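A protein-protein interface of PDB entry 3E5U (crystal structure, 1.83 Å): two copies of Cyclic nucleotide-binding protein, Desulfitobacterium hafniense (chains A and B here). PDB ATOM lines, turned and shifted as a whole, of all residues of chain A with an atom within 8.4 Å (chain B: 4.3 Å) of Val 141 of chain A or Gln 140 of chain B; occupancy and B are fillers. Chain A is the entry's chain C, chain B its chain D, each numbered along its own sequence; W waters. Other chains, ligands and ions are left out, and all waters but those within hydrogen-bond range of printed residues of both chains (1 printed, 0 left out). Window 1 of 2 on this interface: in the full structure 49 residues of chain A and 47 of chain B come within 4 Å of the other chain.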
ATOM      1  N   ILE A  65      22.917  10.834  17.807  1.00  0.00           N
ATOM      2  CA  ILE A  65      22.355  12.043  18.455  1.00  0.00           C
ATOM      3  C   ILE A  65      23.522  12.817  19.095  1.00  0.00           C
ATOM      4  O   ILE A  65      24.534  12.223  19.537  1.00  0.00           O
ATOM      5  CB  ILE A  65      21.269  11.657  19.505  1.00  0.00           C
ATOM      6  CG1 ILE A  65      20.514  12.926  20.001  1.00  0.00           C
ATOM      7  CG2 ILE A  65      21.888  10.739  20.620  1.00  0.00           C
ATOM      8  CD1 ILE A  65      19.264  12.622  21.033  1.00  0.00           C
ATOM      9  N   PHE A  67      24.108  15.936  21.887  1.00  0.00           N
ATOM     10  CA  PHE A  67      23.559  16.862  22.913  1.00  0.00           C
ATOM     11  C   PHE A  67      24.104  18.285  22.856  1.00  0.00           C
ATOM     12  O   PHE A  67      25.035  18.583  22.134  1.00  0.00           O
ATOM     13  CB  PHE A  67      23.659  16.246  24.296  1.00  0.00           C
ATOM     14  CG  PHE A  67      22.786  15.005  24.450  1.00  0.00           C
ATOM     15  CD1 PHE A  67      23.368  13.746  24.583  1.00  0.00           C
ATOM     16  CD2 PHE A  67      21.411  15.133  24.462  1.00  0.00           C
ATOM     17  CE1 PHE A  67      22.577  12.595  24.707  1.00  0.00           C
ATOM     18  CE2 PHE A  67      20.577  13.987  24.590  1.00  0.00           C
ATOM     19  CZ  PHE A  67      21.153  12.730  24.710  1.00  0.00           C
ATOM     20  N   LEU A  75      22.525   6.160  17.736  1.00  0.00           N
ATOM     21  CA  LEU A  75      21.127   5.707  17.715  1.00  0.00           C
ATOM     22  C   LEU A  75      20.992   4.411  16.908  1.00  0.00           C
ATOM     23  O   LEU A  75      20.494   3.392  17.437  1.00  0.00           O
ATOM     24  CB  LEU A  75      20.136   6.740  17.208  1.00  0.00           C
ATOM     25  CG  LEU A  75      19.980   8.009  18.058  1.00  0.00           C
ATOM     26  CD1 LEU A  75      18.787   8.894  17.477  1.00  0.00           C
ATOM     27  CD2 LEU A  75      19.873   7.703  19.554  1.00  0.00           C
ATOM     28  N   ASN A  92      15.717  16.951  18.511  1.00  0.00           N
ATOM     29  CA  ASN A  92      16.998  16.312  18.612  1.00  0.00           C
ATOM     30  C   ASN A  92      17.936  16.798  17.489  1.00  0.00           C
ATOM     31  O   ASN A  92      17.522  16.880  16.333  1.00  0.00           O
ATOM     32  CB  ASN A  92      16.831  14.816  18.540  1.00  0.00           C
ATOM     33  CG  ASN A  92      16.019  14.292  19.703  1.00  0.00           C
ATOM     34  OD1 ASN A  92      16.100  14.846  20.807  1.00  0.00           O
ATOM     35  ND2 ASN A  92      15.245  13.250  19.486  1.00  0.00           N
ATOM     36  N   VAL A 134       9.971   2.438  17.718  1.00  0.00           N
ATOM     37  CA  VAL A 134       9.346   2.710  19.002  1.00  0.00           C
ATOM     38  C   VAL A 134       9.581   1.510  19.955  1.00  0.00           C
ATOM     39  O   VAL A 134       9.985   1.682  21.101  1.00  0.00           O
ATOM     40  CB  VAL A 134       7.844   3.067  18.869  1.00  0.00           C
ATOM     41  CG1 VAL A 134       7.178   3.341  20.309  1.00  0.00           C
ATOM     42  CG2 VAL A 134       7.713   4.344  18.055  1.00  0.00           C
ATOM     43  N   ALA A 135       9.254   0.337  19.470  1.00  0.00           N
ATOM     44  CA  ALA A 135       9.303  -0.908  20.269  1.00  0.00           C
ATOM     45  C   ALA A 135      10.725  -1.175  20.735  1.00  0.00           C
ATOM     46  O   ALA A 135      10.935  -1.478  21.887  1.00  0.00           O
ATOM     47  CB  ALA A 135       8.826  -2.017  19.471  1.00  0.00           C
ATOM     48  N   TYR A 136      11.713  -0.935  19.857  1.00  0.00           N
ATOM     49  CA  TYR A 136      13.111  -1.115  20.189  1.00  0.00           C
ATOM     50  C   TYR A 136      13.528  -0.151  21.348  1.00  0.00           C
ATOM     51  O   TYR A 136      13.998  -0.618  22.401  1.00  0.00           O
ATOM     52  CB  TYR A 136      14.043  -0.990  18.961  1.00  0.00           C
ATOM     53  CG  TYR A 136      15.472  -1.110  19.363  1.00  0.00           C
ATOM     54  CD1 TYR A 136      16.018  -2.400  19.609  1.00  0.00           C
ATOM     55  CD2 TYR A 136      16.237   0.015  19.676  1.00  0.00           C
ATOM     56  CE1 TYR A 136      17.287  -2.567  20.087  1.00  0.00           C
ATOM     57  CE2 TYR A 136      17.574  -0.146  20.163  1.00  0.00           C
ATOM     58  CZ  TYR A 136      18.071  -1.422  20.357  1.00  0.00           C
ATOM     59  OH  TYR A 136      19.356  -1.644  20.818  1.00  0.00           O
ATOM     60  N   TYR A 137      13.408   1.164  21.121  1.00  0.00           N
ATOM     61  CA  TYR A 137      13.905   2.138  22.084  1.00  0.00           C
ATOM     62  C   TYR A 137      13.112   2.195  23.388  1.00  0.00           C
ATOM     63  O   TYR A 137      13.682   2.406  24.413  1.00  0.00           O
ATOM     64  CB  TYR A 137      14.015   3.545  21.440  1.00  0.00           C
ATOM     65  CG  TYR A 137      15.051   3.566  20.315  1.00  0.00           C
ATOM     66  CD1 TYR A 137      14.661   3.726  18.951  1.00  0.00           C
ATOM     67  CD2 TYR A 137      16.446   3.515  20.608  1.00  0.00           C
ATOM     68  CE1 TYR A 137      15.569   3.733  17.918  1.00  0.00           C
ATOM     69  CE2 TYR A 137      17.392   3.515  19.560  1.00  0.00           C
ATOM     70  CZ  TYR A 137      16.949   3.642  18.197  1.00  0.00           C
ATOM     71  OH  TYR A 137      17.864   3.640  17.181  1.00  0.00           O
ATOM     72  N   ALA A 138      11.801   1.994  23.343  1.00  0.00           N
ATOM     73  CA  ALA A 138      10.996   1.907  24.545  1.00  0.00           C
ATOM     74  C   ALA A 138      11.413   0.701  25.401  1.00  0.00           C
ATOM     75  O   ALA A 138      11.606   0.841  26.587  1.00  0.00           O
ATOM     76  CB  ALA A 138       9.521   1.865  24.197  1.00  0.00           C
ATOM     77  N   ARG A 139      11.590  -0.461  24.797  1.00  0.00           N
ATOM     78  CA  ARG A 139      12.079  -1.636  25.522  1.00  0.00           C
ATOM     79  C   ARG A 139      13.459  -1.410  26.096  1.00  0.00           C
ATOM     80  O   ARG A 139      13.701  -1.780  27.238  1.00  0.00           O
ATOM     81  CB  ARG A 139      11.980  -2.896  24.674  1.00  0.00           C
ATOM     82  CG  ARG A 139      12.601  -4.160  25.300  1.00  0.00           C
ATOM     83  CD  ARG A 139      12.767  -5.243  24.224  1.00  0.00           C
ATOM     84  NE  ARG A 139      13.171  -6.529  24.760  1.00  0.00           N
ATOM     85  CZ  ARG A 139      12.389  -7.513  25.257  1.00  0.00           C
ATOM     86  NH1 ARG A 139      11.047  -7.431  25.315  1.00  0.00           N
ATOM     87  NH2 ARG A 139      12.984  -8.628  25.706  1.00  0.00           N
ATOM     88  N   GLN A 140      14.319  -0.717  25.363  1.00  0.00           N
ATOM     89  CA  GLN A 140      15.651  -0.469  25.850  1.00  0.00           C
ATOM     90  C   GLN A 140      15.675   0.437  27.081  1.00  0.00           C
ATOM     91  O   GLN A 140      16.377   0.149  28.019  1.00  0.00           O
ATOM     92  CB  GLN A 140      16.496   0.100  24.725  1.00  0.00           C
ATOM     93  CG  GLN A 140      17.902   0.326  25.109  1.00  0.00           C
ATOM     94  CD  GLN A 140      18.746   0.480  23.863  1.00  0.00           C
ATOM     95  OE1 GLN A 140      19.871  -0.042  23.776  1.00  0.00           O
ATOM     96  NE2 GLN A 140      18.227   1.205  22.898  1.00  0.00           N
ATOM     97  N   VAL A 141      14.901   1.522  27.078  1.00  0.00           N
ATOM     98  CA  VAL A 141      14.718   2.306  28.287  1.00  0.00           C
ATOM     99  C   VAL A 141      14.308   1.438  29.508  1.00  0.00           C
ATOM    100  O   VAL A 141      14.919   1.515  30.607  1.00  0.00           O
ATOM    101  CB  VAL A 141      13.757   3.501  28.083  1.00  0.00           C
ATOM    102  CG1 VAL A 141      13.456   4.146  29.461  1.00  0.00           C
ATOM    103  CG2 VAL A 141      14.309   4.563  27.033  1.00  0.00           C
ATOM    104  N   ALA A 142      13.266   0.627  29.351  1.00  0.00           N
ATOM    105  CA  ALA A 142      12.751  -0.179  30.422  1.00  0.00           C
ATOM    106  C   ALA A 142      13.776  -1.215  30.875  1.00  0.00           C
ATOM    107  O   ALA A 142      13.902  -1.463  32.055  1.00  0.00           O
ATOM    108  CB  ALA A 142      11.492  -0.851  29.976  1.00  0.00           C
ATOM    109  N   GLU A 143      14.470  -1.843  29.933  1.00  0.00           N
ATOM    110  CA  GLU A 143      15.486  -2.855  30.309  1.00  0.00           C
ATOM    111  C   GLU A 143      16.624  -2.207  31.072  1.00  0.00           C
ATOM    112  O   GLU A 143      17.158  -2.805  32.040  1.00  0.00           O
ATOM    113  CB  GLU A 143      16.043  -3.484  29.085  1.00  0.00           C
ATOM    114  CG  GLU A 143      16.924  -4.745  29.353  1.00  0.00           C
ATOM    115  CD  GLU A 143      17.826  -5.095  28.158  1.00  0.00           C
ATOM    116  OE1 GLU A 143      18.458  -6.191  28.164  1.00  0.00           O
ATOM    117  OE2 GLU A 143      17.942  -4.241  27.246  1.00  0.00           O
ATOM    118  N   MET A 144      17.070  -1.024  30.596  1.00  0.00           N
ATOM    119  CA  MET A 144      18.117  -0.291  31.321  1.00  0.00           C
ATOM    120  C   MET A 144      17.714   0.007  32.781  1.00  0.00           C
ATOM    121  O   MET A 144      18.564   0.122  33.677  1.00  0.00           O
ATOM    122  CB  MET A 144      18.505   0.957  30.587  1.00  0.00           C
ATOM    123  CG  MET A 144      19.214   0.657  29.215  1.00  0.00           C
ATOM    124  SD  MET A 144      19.355   2.213  28.225  1.00  0.00           S
ATOM    125  CE  MET A 144      20.748   2.909  29.123  1.00  0.00           C
ATOM    126  N   ASN A 145      16.408   0.105  33.005  1.00  0.00           N
ATOM    127  CA  ASN A 145      15.877   0.364  34.327  1.00  0.00           C
ATOM    128  C   ASN A 145      15.543  -0.894  35.104  1.00  0.00           C
ATOM    129  O   ASN A 145      15.015  -0.790  36.213  1.00  0.00           O
ATOM    130  CB  ASN A 145      14.642   1.302  34.222  1.00  0.00           C
ATOM    131  CG  ASN A 145      15.028   2.749  34.041  1.00  0.00           C
ATOM    132  OD1 ASN A 145      16.048   3.188  34.570  1.00  0.00           O
ATOM    133  ND2 ASN A 145      14.249   3.481  33.260  1.00  0.00           N
ATOM    134  N   THR A 146      15.831  -2.074  34.524  1.00  0.00           N
ATOM    135  CA  THR A 146      15.455  -3.377  35.076  1.00  0.00           C
ATOM    136  C   THR A 146      16.664  -4.293  35.353  1.00  0.00           C
ATOM    137  O   THR A 146      16.731  -4.874  36.417  1.00  0.00           O
ATOM    138  CB  THR A 146      14.450  -4.144  34.184  1.00  0.00           C
ATOM    139  OG1 THR A 146      13.292  -3.320  33.974  1.00  0.00           O
ATOM    140  CG2 THR A 146      14.066  -5.466  34.848  1.00  0.00           C
ATOM    141  N   TYR A 147      17.591  -4.385  34.396  1.00  0.00           N
ATOM    142  CA  TYR A 147      18.623  -5.406  34.354  1.00  0.00           C
ATOM    143  C   TYR A 147      20.003  -4.752  34.476  1.00  0.00           C
ATOM    144  O   TYR A 147      20.237  -3.718  33.883  1.00  0.00           O
ATOM    145  CB  TYR A 147      18.500  -6.214  33.044  1.00  0.00           C
ATOM    146  CG  TYR A 147      17.208  -7.038  33.018  1.00  0.00           C
ATOM    147  CD1 TYR A 147      16.993  -8.051  33.968  1.00  0.00           C
ATOM    148  CD2 TYR A 147      16.187  -6.739  32.149  1.00  0.00           C
ATOM    149  CE1 TYR A 147      15.811  -8.740  34.000  1.00  0.00           C
ATOM    150  CE2 TYR A 147      14.974  -7.443  32.183  1.00  0.00           C
ATOM    151  CZ  TYR A 147      14.792  -8.421  33.115  1.00  0.00           C
ATOM    152  OH  TYR A 147      13.609  -9.143  33.109  1.00  0.00           O
ATOM    153  N   ARG A 152      22.163  -7.511  30.890  1.00  0.00           N
ATOM    154  CA  ARG A 152      21.899  -6.940  29.539  1.00  0.00           C
ATOM    155  C   ARG A 152      22.793  -7.531  28.421  1.00  0.00           C
ATOM    156  O   ARG A 152      22.295  -7.815  27.337  1.00  0.00           O
ATOM    157  CB  ARG A 152      21.972  -5.389  29.555  1.00  0.00           C
ATOM    158  CG  ARG A 152      20.913  -4.771  30.423  1.00  0.00           C
ATOM    159  CD  ARG A 152      20.597  -3.281  30.151  1.00  0.00           C
ATOM    160  NE  ARG A 152      21.723  -2.354  30.070  1.00  0.00           N
ATOM    161  CZ  ARG A 152      22.253  -1.685  31.096  1.00  0.00           C
ATOM    162  NH1 ARG A 152      21.801  -1.865  32.321  1.00  0.00           N
ATOM    163  NH2 ARG A 152      23.268  -0.842  30.899  1.00  0.00           N
ATOM    164  N   TYR B 136      11.474  10.652  21.335  1.00  0.00           N
ATOM    165  CA  TYR B 136      11.412  10.543  22.803  1.00  0.00           C
ATOM    166  C   TYR B 136      12.318   9.415  23.363  1.00  0.00           C
ATOM    167  O   TYR B 136      13.260   9.683  24.142  1.00  0.00           O
ATOM    168  CB  TYR B 136       9.934  10.520  23.368  1.00  0.00           C
ATOM    169  CG  TYR B 136      10.021  10.432  24.909  1.00  0.00           C
ATOM    170  CD1 TYR B 136      10.247  11.583  25.679  1.00  0.00           C
ATOM    171  CD2 TYR B 136      10.068   9.200  25.524  1.00  0.00           C
ATOM    172  CE1 TYR B 136      10.438  11.520  27.058  1.00  0.00           C
ATOM    173  CE2 TYR B 136      10.312   9.097  26.923  1.00  0.00           C
ATOM    174  CZ  TYR B 136      10.516  10.260  27.668  1.00  0.00           C
ATOM    175  OH  TYR B 136      10.696  10.183  29.030  1.00  0.00           O
ATOM    176  N   TYR B 137      12.022   8.168  23.034  1.00  0.00           N
ATOM    177  CA  TYR B 137      12.701   7.010  23.610  1.00  0.00           C
ATOM    178  C   TYR B 137      14.141   6.905  23.189  1.00  0.00           C
ATOM    179  O   TYR B 137      14.933   6.456  23.977  1.00  0.00           O
ATOM    180  CB  TYR B 137      11.940   5.725  23.312  1.00  0.00           C
ATOM    181  CG  TYR B 137      10.562   5.711  24.013  1.00  0.00           C
ATOM    182  CD1 TYR B 137       9.368   5.839  23.274  1.00  0.00           C
ATOM    183  CD2 TYR B 137      10.468   5.580  25.418  1.00  0.00           C
ATOM    184  CE1 TYR B 137       8.100   5.839  23.945  1.00  0.00           C
ATOM    185  CE2 TYR B 137       9.239   5.573  26.064  1.00  0.00           C
ATOM    186  CZ  TYR B 137       8.056   5.678  25.345  1.00  0.00           C
ATOM    187  OH  TYR B 137       6.861   5.702  26.062  1.00  0.00           O
ATOM    188  N   ALA B 138      14.409   7.179  21.887  1.00  0.00           N
ATOM    189  CA  ALA B 138      15.824   7.206  21.345  1.00  0.00           C
ATOM    190  C   ALA B 138      16.681   8.211  22.123  1.00  0.00           C
ATOM    191  O   ALA B 138      17.694   7.805  22.635  1.00  0.00           O
ATOM    192  CB  ALA B 138      15.883   7.461  19.851  1.00  0.00           C
ATOM    193  N   ARG B 139      16.223   9.461  22.284  1.00  0.00           N
ATOM    194  CA  ARG B 139      16.903  10.439  23.192  1.00  0.00           C
ATOM    195  C   ARG B 139      17.064   9.932  24.610  1.00  0.00           C
ATOM    196  O   ARG B 139      18.128  10.083  25.211  1.00  0.00           O
ATOM    197  CB  ARG B 139      16.105  11.730  23.267  1.00  0.00           C
ATOM    198  CG  ARG B 139      16.855  12.952  23.743  1.00  0.00           C
ATOM    199  CD  ARG B 139      15.922  14.146  23.894  1.00  0.00           C
ATOM    200  NE  ARG B 139      16.535  15.252  24.603  1.00  0.00           N
ATOM    201  CZ  ARG B 139      17.236  16.263  24.088  1.00  0.00           C
ATOM    202  NH1 ARG B 139      17.518  16.356  22.767  1.00  0.00           N
ATOM    203  NH2 ARG B 139      17.726  17.178  24.942  1.00  0.00           N
ATOM    204  N   GLN B 140      15.973   9.414  25.189  1.00  0.00           N
ATOM    205  CA  GLN B 140      16.020   8.914  26.580  1.00  0.00           C
ATOM    206  C   GLN B 140      17.128   7.844  26.808  1.00  0.00           C
ATOM    207  O   GLN B 140      17.824   7.919  27.808  1.00  0.00           O
ATOM    208  CB  GLN B 140      14.659   8.366  27.000  1.00  0.00           C
ATOM    209  CG  GLN B 140      14.489   8.192  28.470  1.00  0.00           C
ATOM    210  CD  GLN B 140      14.601   9.509  29.262  1.00  0.00           C
ATOM    211  OE1 GLN B 140      14.345  10.610  28.734  1.00  0.00           O
ATOM    212  NE2 GLN B 140      15.037   9.401  30.505  1.00  0.00           N
ATOM    213  N   VAL B 141      17.275   6.869  25.907  1.00  0.00           N
ATOM    214  CA  VAL B 141      18.374   5.855  25.968  1.00  0.00           C
ATOM    215  C   VAL B 141      19.763   6.506  26.028  1.00  0.00           C
ATOM    216  O   VAL B 141      20.560   6.238  26.955  1.00  0.00           O
ATOM    217  CB  VAL B 141      18.304   4.901  24.777  1.00  0.00           C
ATOM    218  CG1 VAL B 141      19.568   3.991  24.739  1.00  0.00           C
ATOM    219  CG2 VAL B 141      17.004   4.129  24.832  1.00  0.00           C
ATOM    220  N   ALA B 142      19.976   7.413  25.068  1.00  0.00           N
ATOM    221  CA  ALA B 142      21.175   8.212  24.966  1.00  0.00           C
ATOM    222  C   ALA B 142      21.422   9.059  26.221  1.00  0.00           C
ATOM    223  O   ALA B 142      22.519   9.105  26.740  1.00  0.00           O
ATOM    224  CB  ALA B 142      21.126   9.089  23.702  1.00  0.00           C
ATOM    225  N   GLU B 143      20.391   9.720  26.713  1.00  0.00           N
ATOM    226  CA  GLU B 143      20.562  10.496  27.939  1.00  0.00           C
ATOM    227  C   GLU B 143      20.909   9.620  29.156  1.00  0.00           C
ATOM    228  O   GLU B 143      21.769   9.940  29.996  1.00  0.00           O
ATOM    229  CB  GLU B 143      19.293  11.284  28.162  1.00  0.00           C
ATOM    230  CG  GLU B 143      19.441  12.399  29.163  1.00  0.00           C
ATOM    231  CD  GLU B 143      18.192  13.199  29.294  1.00  0.00           C
ATOM    232  OE1 GLU B 143      18.147  13.933  30.331  1.00  0.00           O
ATOM    233  OE2 GLU B 143      17.259  13.064  28.395  1.00  0.00           O
ATOM    234  N   MET B 144      20.243   8.500  29.281  1.00  0.00           N
ATOM    235  CA  MET B 144      20.585   7.568  30.346  1.00  0.00           C
ATOM    236  C   MET B 144      22.061   7.101  30.257  1.00  0.00           C
ATOM    237  O   MET B 144      22.702   6.808  31.269  1.00  0.00           O
ATOM    238  CB  MET B 144      19.580   6.378  30.309  1.00  0.00           C
ATOM    239  CG  MET B 144      18.182   6.770  30.722  1.00  0.00           C
ATOM    240  SD  MET B 144      17.003   5.485  30.330  1.00  0.00           S
ATOM    241  CE  MET B 144      17.496   4.248  31.563  1.00  0.00           C
ATOM    242  N   ILE B 186       9.980   8.153  35.059  1.00  0.00           N
ATOM    243  CA  ILE B 186      10.359   8.772  33.755  1.00  0.00           C
ATOM    244  C   ILE B 186      11.872   8.886  33.593  1.00  0.00           C
ATOM    245  O   ILE B 186      12.403   8.563  32.519  1.00  0.00           O
ATOM    246  CB  ILE B 186       9.786  10.222  33.584  1.00  0.00           C
ATOM    247  CG1 ILE B 186       8.246  10.224  33.501  1.00  0.00           C
ATOM    248  CG2 ILE B 186      10.393  10.936  32.372  1.00  0.00           C
ATOM    249  CD1 ILE B 186       7.661  11.653  33.612  1.00  0.00           C
HETATM  250  O   HOH W   1      14.481   6.407  32.379  1.00  0.00           O
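CG2 of Ile 65 of chain A touches CB of Ala 142 of chain B (3.6 Å). Phe 67 of chain A touches Arg 139 of chain B (CE2 to CG, 3.95 Å). Glu 143 of chain B touches Phe 67 of chain A. Leu 75 of chain A touches Ala 138 of chain B (CD2 to O, 3.8 Å). Tyr 137 of chain B touches Tyr 137 of chain A. Val 141 of chain B touches Tyr 137 of chain A (CG2 to O, 3.8 Å). Tyr 137 of chain B touches Ala 138 of chain A. Val 141 of chain B touches Gln 140 of chain A (CG1 to NE2, 3.6 Å). Met 144 of chain A touches Val 141 of chain B (SD to CG1, 3.9 Å). Met 144 of chain B touches Met 144 of chain A.
The side-chain amide nitrogen (NE2) of Gln 140 of chain B is in hydrogen-bond range of the backbone carbonyl oxygen (O) of Ile 186 of chain B, at 3.4 Å. The side-chain amide nitrogen (ND2) of Asn 145 of chain A lies within hydrogen-bond range of the backbone carbonyl oxygen (O) of Val 141 of chain A (3.4 Å). The side-chain hydroxyl (OH) of Tyr 136 of chain A sits at hydrogen-bond distance from the side-chain amide oxygen (OE1) of Gln 140 of chain A. OH of Tyr 137 of chain A is in hydrogen-bond range of O of Leu 75 of chain A, 2.7 Å away.
Printed residues of chain B within 4 Å of Ile 65 of chain A: Arg 139 (3.6 Å) and Ala 142 (3.6 Å). Printed residues of chain B within 4 Å of Phe 67 of chain A: Arg 139 (3.95 Å), Ala 142 (3.8 Å) and Glu 143 (3.7 Å). Of the printed residues of chain B, Gln 140 of chain A touches Val 141 (3.6 Å). Printed residues of chain A within 4 Å of Ala 138 of chain B: Leu 75 and Tyr 137. Printed residues of chain A within 4 Å of Gln 140 of chain B: Val 141. Printed residues of chain A within 4 Å of Glu 143 of chain B: Phe 67. The nearest printed residue of chain B that does not touch Val 141 of chain A is Ile 186 of chain B (5.5 Å). The nearest residue of chain A that does not touch Gln 140 of chain B is Met 144 of chain A (5.9 Å).
Water W1 lies within hydrogen-bond range of the backbone carbonyl oxygen of Ile 186 of chain B, the side-chain amide nitrogen of Asn 145 of chain A and the side-chain sulfur of Met 144 of chain B.
OD1 of Asn 92 of chain A lies within hydrogen-bond range of NH1 of Arg 139 of chain B, 2.9 Å away.
Tyr 137 of chain A touches Ala 138 of chain B, and with the chains exchanged Ala 138 of chain A touches Tyr 137 of chain B. Tyr 137 of chain A touches Val 141 of chain B, and with the chains exchanged Val 141 of chain A touches Tyr 137 of chain B. Val 141 of chain B touches its own counterpart, Val 141 of chain A. Val 141 of chain A touches Met 144 of chain B, and with the chains exchanged Met 144 of chain A touches Val 141 of chain B. Positions printed for both chains: 136, 137, 138, 139, 140, 141, 142, 143 and 144. Of the 19 pairs that touch across the chains among the printed residues, 11 have their exchanged pair printed and touching as well.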
